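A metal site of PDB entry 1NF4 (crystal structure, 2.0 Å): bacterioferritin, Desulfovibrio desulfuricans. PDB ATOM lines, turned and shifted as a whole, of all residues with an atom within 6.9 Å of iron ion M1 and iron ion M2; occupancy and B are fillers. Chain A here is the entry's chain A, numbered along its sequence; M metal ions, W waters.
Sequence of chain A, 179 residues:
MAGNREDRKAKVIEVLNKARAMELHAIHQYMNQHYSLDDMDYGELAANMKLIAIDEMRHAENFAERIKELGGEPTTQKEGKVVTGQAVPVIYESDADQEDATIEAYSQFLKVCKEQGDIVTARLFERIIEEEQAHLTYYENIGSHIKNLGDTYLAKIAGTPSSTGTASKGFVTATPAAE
OE2 of Glu 99 lies close to OH of Tyr 30 (2.7 Å). The side-chain carboxylate (OE1) of Glu 131 lies within hydrogen-bond range of a ring nitrogen (NE2) of His 59. OE2 of Glu 23 sits close to OH of Tyr 106 (2.5 Å). A ring nitrogen (NE2) of His 135 lies within hydrogen-bond range of the side-chain carboxylate of Asp 55, 2.8 Å away.
Of the 23 residues printed, 4 come within 4 Å of iron ion M2. Along chain A the residues within 4 Å of iron ion M2 span positions 23 to 132.
Iron ion M2 is bound by the side-chain carboxylate (OE2) of Glu 132, the side-chain carboxylate (OE1) of Glu 56, a ring nitrogen (ND1) of His 59, the side-chain carboxylate (OE2) of Glu 23, the side-chain carboxylate (OE1) of Glu 23 and water W1.
Iron ion M1 is bound by the side-chain carboxylate (OE1) of Glu 132 (2.0 Å), the side-chain carboxylate (OE2) of Glu 56 (2.1 Å), the side-chain carboxylate (OE2) of Glu 99 (2.2 Å), a ring nitrogen (ND1) of His 135 (2.3 Å) and the side-chain carboxylate (OE1) of Glu 99 (2.5 Å). Iron ion M1 has five donor atoms within binding distance.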
ATOM      1  N   ALA A  19       4.523  -2.225  27.637  1.00  0.00           N
ATOM      2  CA  ALA A  19       4.996  -0.945  28.162  1.00  0.00           C
ATOM      3  C   ALA A  19       6.140  -0.428  27.287  1.00  0.00           C
ATOM      4  O   ALA A  19       6.193   0.737  26.890  1.00  0.00           O
ATOM      5  CB  ALA A  19       5.451  -1.088  29.601  1.00  0.00           C
ATOM      6  N   MET A  22       5.077   1.009  24.110  1.00  0.00           N
ATOM      7  CA  MET A  22       4.559   2.334  24.443  1.00  0.00           C
ATOM      8  C   MET A  22       5.705   3.337  24.578  1.00  0.00           C
ATOM      9  O   MET A  22       5.551   4.461  24.090  1.00  0.00           O
ATOM     10  CB  MET A  22       3.730   2.277  25.720  1.00  0.00           C
ATOM     11  CG  MET A  22       2.346   1.663  25.455  1.00  0.00           C
ATOM     12  SD  MET A  22       1.467   1.373  26.994  1.00  0.00           S
ATOM     13  CE  MET A  22       0.886   2.998  27.414  1.00  0.00           C
ATOM     14  N   GLU A  23       6.812   2.951  25.186  1.00  0.00           N
ATOM     15  CA  GLU A  23       7.982   3.833  25.282  1.00  0.00           C
ATOM     16  C   GLU A  23       8.548   4.139  23.899  1.00  0.00           C
ATOM     17  O   GLU A  23       8.871   5.278  23.566  1.00  0.00           O
ATOM     18  CB  GLU A  23       9.089   3.213  26.140  1.00  0.00           C
ATOM     19  CG  GLU A  23       8.739   2.988  27.603  1.00  0.00           C
ATOM     20  CD  GLU A  23       8.484   4.277  28.351  1.00  0.00           C
ATOM     21  OE1 GLU A  23       8.937   5.353  27.893  1.00  0.00           O
ATOM     22  OE2 GLU A  23       7.828   4.228  29.412  1.00  0.00           O
ATOM     23  N   ALA A  26       6.552   6.724  22.261  1.00  0.00           N
ATOM     24  CA  ALA A  26       6.768   8.039  22.858  1.00  0.00           C
ATOM     25  C   ALA A  26       8.079   8.669  22.413  1.00  0.00           C
ATOM     26  O   ALA A  26       8.154   9.864  22.154  1.00  0.00           O
ATOM     27  CB  ALA A  26       6.736   7.948  24.381  1.00  0.00           C
ATOM     28  N   TYR A  30       7.662  12.183  20.562  1.00  0.00           N
ATOM     29  CA  TYR A  30       8.290  13.329  21.209  1.00  0.00           C
ATOM     30  C   TYR A  30       9.440  13.868  20.373  1.00  0.00           C
ATOM     31  O   TYR A  30       9.617  15.084  20.266  1.00  0.00           O
ATOM     32  CB  TYR A  30       8.788  12.971  22.620  1.00  0.00           C
ATOM     33  CG  TYR A  30       7.652  12.600  23.564  1.00  0.00           C
ATOM     34  CD1 TYR A  30       7.909  11.924  24.747  1.00  0.00           C
ATOM     35  CD2 TYR A  30       6.341  12.929  23.242  1.00  0.00           C
ATOM     36  CE1 TYR A  30       6.876  11.576  25.606  1.00  0.00           C
ATOM     37  CE2 TYR A  30       5.296  12.600  24.092  1.00  0.00           C
ATOM     38  CZ  TYR A  30       5.578  11.926  25.265  1.00  0.00           C
ATOM     39  OH  TYR A  30       4.559  11.578  26.119  1.00  0.00           O
ATOM     40  N   ILE A  52      12.819  14.843  27.650  1.00  0.00           N
ATOM     41  CA  ILE A  52      11.799  13.858  28.037  1.00  0.00           C
ATOM     42  C   ILE A  52      11.874  12.635  27.130  1.00  0.00           C
ATOM     43  O   ILE A  52      11.748  11.509  27.621  1.00  0.00           O
ATOM     44  CB  ILE A  52      10.382  14.467  28.041  1.00  0.00           C
ATOM     45  CG1 ILE A  52      10.189  15.479  29.174  1.00  0.00           C
ATOM     46  CG2 ILE A  52       9.310  13.402  28.087  1.00  0.00           C
ATOM     47  CD1 ILE A  52       8.908  16.272  29.072  1.00  0.00           C
ATOM     48  N   ASP A  55      14.350  10.488  28.636  1.00  0.00           N
ATOM     49  CA  ASP A  55      13.796   9.727  29.752  1.00  0.00           C
ATOM     50  C   ASP A  55      13.040   8.493  29.228  1.00  0.00           C
ATOM     51  O   ASP A  55      13.117   7.436  29.822  1.00  0.00           O
ATOM     52  CB  ASP A  55      12.807  10.525  30.597  1.00  0.00           C
ATOM     53  CG  ASP A  55      13.395  11.604  31.462  1.00  0.00           C
ATOM     54  OD1 ASP A  55      14.624  11.690  31.646  1.00  0.00           O
ATOM     55  OD2 ASP A  55      12.585  12.411  32.007  1.00  0.00           O
ATOM     56  N   GLU A  56      12.296   8.635  28.123  1.00  0.00           N
ATOM     57  CA  GLU A  56      11.547   7.496  27.578  1.00  0.00           C
ATOM     58  C   GLU A  56      12.481   6.432  27.013  1.00  0.00           C
ATOM     59  O   GLU A  56      12.194   5.236  27.136  1.00  0.00           O
ATOM     60  CB  GLU A  56      10.556   7.926  26.495  1.00  0.00           C
ATOM     61  CG  GLU A  56       9.690   9.119  26.828  1.00  0.00           C
ATOM     62  CD  GLU A  56       8.759   8.973  28.006  1.00  0.00           C
ATOM     63  OE1 GLU A  56       8.965   8.175  28.938  1.00  0.00           O
ATOM     64  OE2 GLU A  56       7.758   9.716  28.048  1.00  0.00           O
ATOM     65  N   MET A  57      13.606   6.829  26.438  1.00  0.00           N
ATOM     66  CA  MET A  57      14.639   5.889  26.012  1.00  0.00           C
ATOM     67  C   MET A  57      15.145   5.082  27.207  1.00  0.00           C
ATOM     68  O   MET A  57      15.267   3.860  27.107  1.00  0.00           O
ATOM     69  CB  MET A  57      15.819   6.584  25.360  1.00  0.00           C
ATOM     70  CG  MET A  57      15.491   7.370  24.111  1.00  0.00           C
ATOM     71  SD  MET A  57      16.834   8.431  23.571  1.00  0.00           S
ATOM     72  CE  MET A  57      15.966   9.682  22.618  1.00  0.00           C
ATOM     73  N   HIS A  59      13.515   4.465  29.961  1.00  0.00           N
ATOM     74  CA  HIS A  59      12.443   3.558  30.387  1.00  0.00           C
ATOM     75  C   HIS A  59      12.438   2.322  29.506  1.00  0.00           C
ATOM     76  O   HIS A  59      12.323   1.178  29.944  1.00  0.00           O
ATOM     77  CB  HIS A  59      11.080   4.245  30.348  1.00  0.00           C
ATOM     78  CG  HIS A  59      10.906   5.387  31.297  1.00  0.00           C
ATOM     79  ND1 HIS A  59       9.849   6.269  31.221  1.00  0.00           N
ATOM     80  CD2 HIS A  59      11.672   5.806  32.345  1.00  0.00           C
ATOM     81  CE1 HIS A  59       9.972   7.174  32.189  1.00  0.00           C
ATOM     82  NE2 HIS A  59      11.064   6.908  32.876  1.00  0.00           N
ATOM     83  N   ALA A  60      12.585   2.531  28.203  1.00  0.00           N
ATOM     84  CA  ALA A  60      12.586   1.391  27.277  1.00  0.00           C
ATOM     85  C   ALA A  60      13.719   0.433  27.613  1.00  0.00           C
ATOM     86  O   ALA A  60      13.554  -0.781  27.617  1.00  0.00           O
ATOM     87  CB  ALA A  60      12.709   1.873  25.842  1.00  0.00           C
ATOM     88  N   PHE A  63      12.873  -1.454  30.945  1.00  0.00           N
ATOM     89  CA  PHE A  63      11.958  -2.559  30.641  1.00  0.00           C
ATOM     90  C   PHE A  63      12.667  -3.711  29.951  1.00  0.00           C
ATOM     91  O   PHE A  63      12.496  -4.874  30.301  1.00  0.00           O
ATOM     92  CB  PHE A  63      10.801  -2.054  29.772  1.00  0.00           C
ATOM     93  CG  PHE A  63       9.826  -1.160  30.512  1.00  0.00           C
ATOM     94  CD1 PHE A  63       9.358   0.014  29.950  1.00  0.00           C
ATOM     95  CD2 PHE A  63       9.402  -1.516  31.782  1.00  0.00           C
ATOM     96  CE1 PHE A  63       8.472   0.799  30.668  1.00  0.00           C
ATOM     97  CE2 PHE A  63       8.505  -0.743  32.488  1.00  0.00           C
ATOM     98  CZ  PHE A  63       8.037   0.430  31.925  1.00  0.00           C
ATOM     99  N   GLN A  98      -1.429  11.594  26.327  1.00  0.00           N
ATOM    100  CA  GLN A  98      -0.667  10.338  26.243  1.00  0.00           C
ATOM    101  C   GLN A  98      -0.020   9.974  27.566  1.00  0.00           C
ATOM    102  O   GLN A  98      -0.125   8.814  27.989  1.00  0.00           O
ATOM    103  CB  GLN A  98       0.398  10.478  25.155  1.00  0.00           C
ATOM    104  CG  GLN A  98       1.201   9.212  24.901  1.00  0.00           C
ATOM    105  CD  GLN A  98       2.277   9.472  23.845  1.00  0.00           C
ATOM    106  OE1 GLN A  98       1.979   9.509  22.656  1.00  0.00           O
ATOM    107  NE2 GLN A  98       3.526   9.633  24.290  1.00  0.00           N
ATOM    108  N   GLU A  99       0.631  10.913  28.255  1.00  0.00           N
ATOM    109  CA  GLU A  99       1.232  10.651  29.558  1.00  0.00           C
ATOM    110  C   GLU A  99       0.188  10.095  30.527  1.00  0.00           C
ATOM    111  O   GLU A  99       0.434   9.181  31.308  1.00  0.00           O
ATOM    112  CB  GLU A  99       1.871  11.906  30.156  1.00  0.00           C
ATOM    113  CG  GLU A  99       3.127  12.388  29.445  1.00  0.00           C
ATOM    114  CD  GLU A  99       4.294  11.431  29.576  1.00  0.00           C
ATOM    115  OE1 GLU A  99       4.276  10.585  30.491  1.00  0.00           O
ATOM    116  OE2 GLU A  99       5.252  11.492  28.764  1.00  0.00           O
ATOM    117  N   THR A 102      -0.635   6.675  29.577  1.00  0.00           N
ATOM    118  CA  THR A 102       0.457   5.802  29.999  1.00  0.00           C
ATOM    119  C   THR A 102       0.394   5.462  31.476  1.00  0.00           C
ATOM    120  O   THR A 102       0.563   4.304  31.880  1.00  0.00           O
ATOM    121  CB  THR A 102       1.816   6.465  29.683  1.00  0.00           C
ATOM    122  OG1 THR A 102       1.935   6.516  28.258  1.00  0.00           O
ATOM    123  CG2 THR A 102       2.985   5.642  30.195  1.00  0.00           C
ATOM    124  N   TYR A 106       0.261   1.640  32.795  1.00  0.00           N
ATOM    125  CA  TYR A 106       1.339   1.119  33.616  1.00  0.00           C
ATOM    126  C   TYR A 106       0.806   0.708  34.987  1.00  0.00           C
ATOM    127  O   TYR A 106       1.277  -0.256  35.573  1.00  0.00           O
ATOM    128  CB  TYR A 106       2.460   2.150  33.789  1.00  0.00           C
ATOM    129  CG  TYR A 106       3.302   2.369  32.553  1.00  0.00           C
ATOM    130  CD1 TYR A 106       2.919   1.857  31.320  1.00  0.00           C
ATOM    131  CD2 TYR A 106       4.497   3.084  32.625  1.00  0.00           C
ATOM    132  CE1 TYR A 106       3.687   2.052  30.182  1.00  0.00           C
ATOM    133  CE2 TYR A 106       5.273   3.276  31.490  1.00  0.00           C
ATOM    134  CZ  TYR A 106       4.878   2.771  30.267  1.00  0.00           C
ATOM    135  OH  TYR A 106       5.652   2.967  29.145  1.00  0.00           O
ATOM    136  N   ILE A 128       8.890   4.097  37.396  1.00  0.00           N
ATOM    137  CA  ILE A 128       8.718   4.780  36.099  1.00  0.00           C
ATOM    138  C   ILE A 128       7.424   5.583  36.082  1.00  0.00           C
ATOM    139  O   ILE A 128       7.355   6.670  35.495  1.00  0.00           O
ATOM    140  CB  ILE A 128       8.844   3.734  34.964  1.00  0.00           C
ATOM    141  CG1 ILE A 128      10.277   3.227  34.785  1.00  0.00           C
ATOM    142  CG2 ILE A 128       8.301   4.268  33.646  1.00  0.00           C
ATOM    143  CD1 ILE A 128      10.482   2.111  33.803  1.00  0.00           C
ATOM    144  N   GLU A 131       7.948   9.020  37.282  1.00  0.00           N
ATOM    145  CA  GLU A 131       8.594   9.861  36.281  1.00  0.00           C
ATOM    146  C   GLU A 131       7.592  10.307  35.213  1.00  0.00           C
ATOM    147  O   GLU A 131       7.646  11.449  34.755  1.00  0.00           O
ATOM    148  CB  GLU A 131       9.772   9.122  35.638  1.00  0.00           C
ATOM    149  CG  GLU A 131      10.742   8.608  36.692  1.00  0.00           C
ATOM    150  CD  GLU A 131      12.045   8.090  36.117  1.00  0.00           C
ATOM    151  OE1 GLU A 131      12.121   7.792  34.911  1.00  0.00           O
ATOM    152  OE2 GLU A 131      13.011   7.956  36.895  1.00  0.00           O
ATOM    153  N   GLU A 132       6.686   9.402  34.831  1.00  0.00           N
ATOM    154  CA  GLU A 132       5.634   9.798  33.898  1.00  0.00           C
ATOM    155  C   GLU A 132       4.782  10.916  34.508  1.00  0.00           C
ATOM    156  O   GLU A 132       4.327  11.803  33.791  1.00  0.00           O
ATOM    157  CB  GLU A 132       4.742   8.635  33.489  1.00  0.00           C
ATOM    158  CG  GLU A 132       5.404   7.386  32.972  1.00  0.00           C
ATOM    159  CD  GLU A 132       6.264   7.545  31.752  1.00  0.00           C
ATOM    160  OE1 GLU A 132       6.425   8.670  31.254  1.00  0.00           O
ATOM    161  OE2 GLU A 132       6.817   6.538  31.255  1.00  0.00           O
ATOM    162  N   GLN A 133       4.590  10.871  35.824  1.00  0.00           N
ATOM    163  CA  GLN A 133       3.817  11.931  36.470  1.00  0.00           C
ATOM    164  C   GLN A 133       4.555  13.257  36.339  1.00  0.00           C
ATOM    165  O   GLN A 133       3.908  14.293  36.170  1.00  0.00           O
ATOM    166  CB  GLN A 133       3.544  11.618  37.940  1.00  0.00           C
ATOM    167  CG  GLN A 133       2.895  12.729  38.739  1.00  0.00           C
ATOM    168  CD  GLN A 133       1.509  13.100  38.252  1.00  0.00           C
ATOM    169  OE1 GLN A 133       0.562  12.321  38.336  1.00  0.00           O
ATOM    170  NE2 GLN A 133       1.344  14.304  37.713  1.00  0.00           N
ATOM    171  N   HIS A 135       6.444  14.059  33.814  1.00  0.00           N
ATOM    172  CA  HIS A 135       6.199  14.430  32.429  1.00  0.00           C
ATOM    173  C   HIS A 135       4.808  15.031  32.245  1.00  0.00           C
ATOM    174  O   HIS A 135       4.669  16.100  31.649  1.00  0.00           O
ATOM    175  CB  HIS A 135       6.367  13.222  31.492  1.00  0.00           C
ATOM    176  CG  HIS A 135       7.741  12.625  31.497  1.00  0.00           C
ATOM    177  ND1 HIS A 135       8.023  11.390  30.964  1.00  0.00           N
ATOM    178  CD2 HIS A 135       8.914  13.097  31.976  1.00  0.00           C
ATOM    179  CE1 HIS A 135       9.299  11.106  31.104  1.00  0.00           C
ATOM    180  NE2 HIS A 135       9.862  12.138  31.721  1.00  0.00           N
ATOM    181  N   LEU A 136       3.772  14.347  32.742  1.00  0.00           N
ATOM    182  CA  LEU A 136       2.395  14.830  32.653  1.00  0.00           C
ATOM    183  C   LEU A 136       2.276  16.250  33.167  1.00  0.00           C
ATOM    184  O   LEU A 136       1.777  17.151  32.497  1.00  0.00           O
ATOM    185  CB  LEU A 136       1.483  13.891  33.441  1.00  0.00           C
ATOM    186  CG  LEU A 136       0.014  14.260  33.642  1.00  0.00           C
ATOM    187  CD1 LEU A 136      -0.655  14.627  32.321  1.00  0.00           C
ATOM    188  CD2 LEU A 136      -0.732  13.105  34.292  1.00  0.00           C
ATOM    189  N   TYR A 139       3.786  18.737  30.751  1.00  0.00           N
ATOM    190  CA  TYR A 139       3.004  19.045  29.539  1.00  0.00           C
ATOM    191  C   TYR A 139       1.758  19.847  29.881  1.00  0.00           C
ATOM    192  O   TYR A 139       1.336  20.735  29.133  1.00  0.00           O
ATOM    193  CB  TYR A 139       2.650  17.751  28.808  1.00  0.00           C
ATOM    194  CG  TYR A 139       3.812  17.091  28.099  1.00  0.00           C
ATOM    195  CD1 TYR A 139       4.093  15.738  28.287  1.00  0.00           C
ATOM    196  CD2 TYR A 139       4.632  17.812  27.249  1.00  0.00           C
ATOM    197  CE1 TYR A 139       5.154  15.137  27.643  1.00  0.00           C
ATOM    198  CE2 TYR A 139       5.702  17.219  26.590  1.00  0.00           C
ATOM    199  CZ  TYR A 139       5.959  15.882  26.797  1.00  0.00           C
ATOM    200  OH  TYR A 139       7.019  15.272  26.149  1.00  0.00           O
HETATM  201 FE    FE M   1       6.576  10.087  29.787  1.00  0.00          FE
HETATM  202 FE    FE M   2       8.183   6.414  29.740  1.00  0.00          FE
HETATM  203  O   HOH W   1       6.519   6.684  28.052  1.00  0.00           O
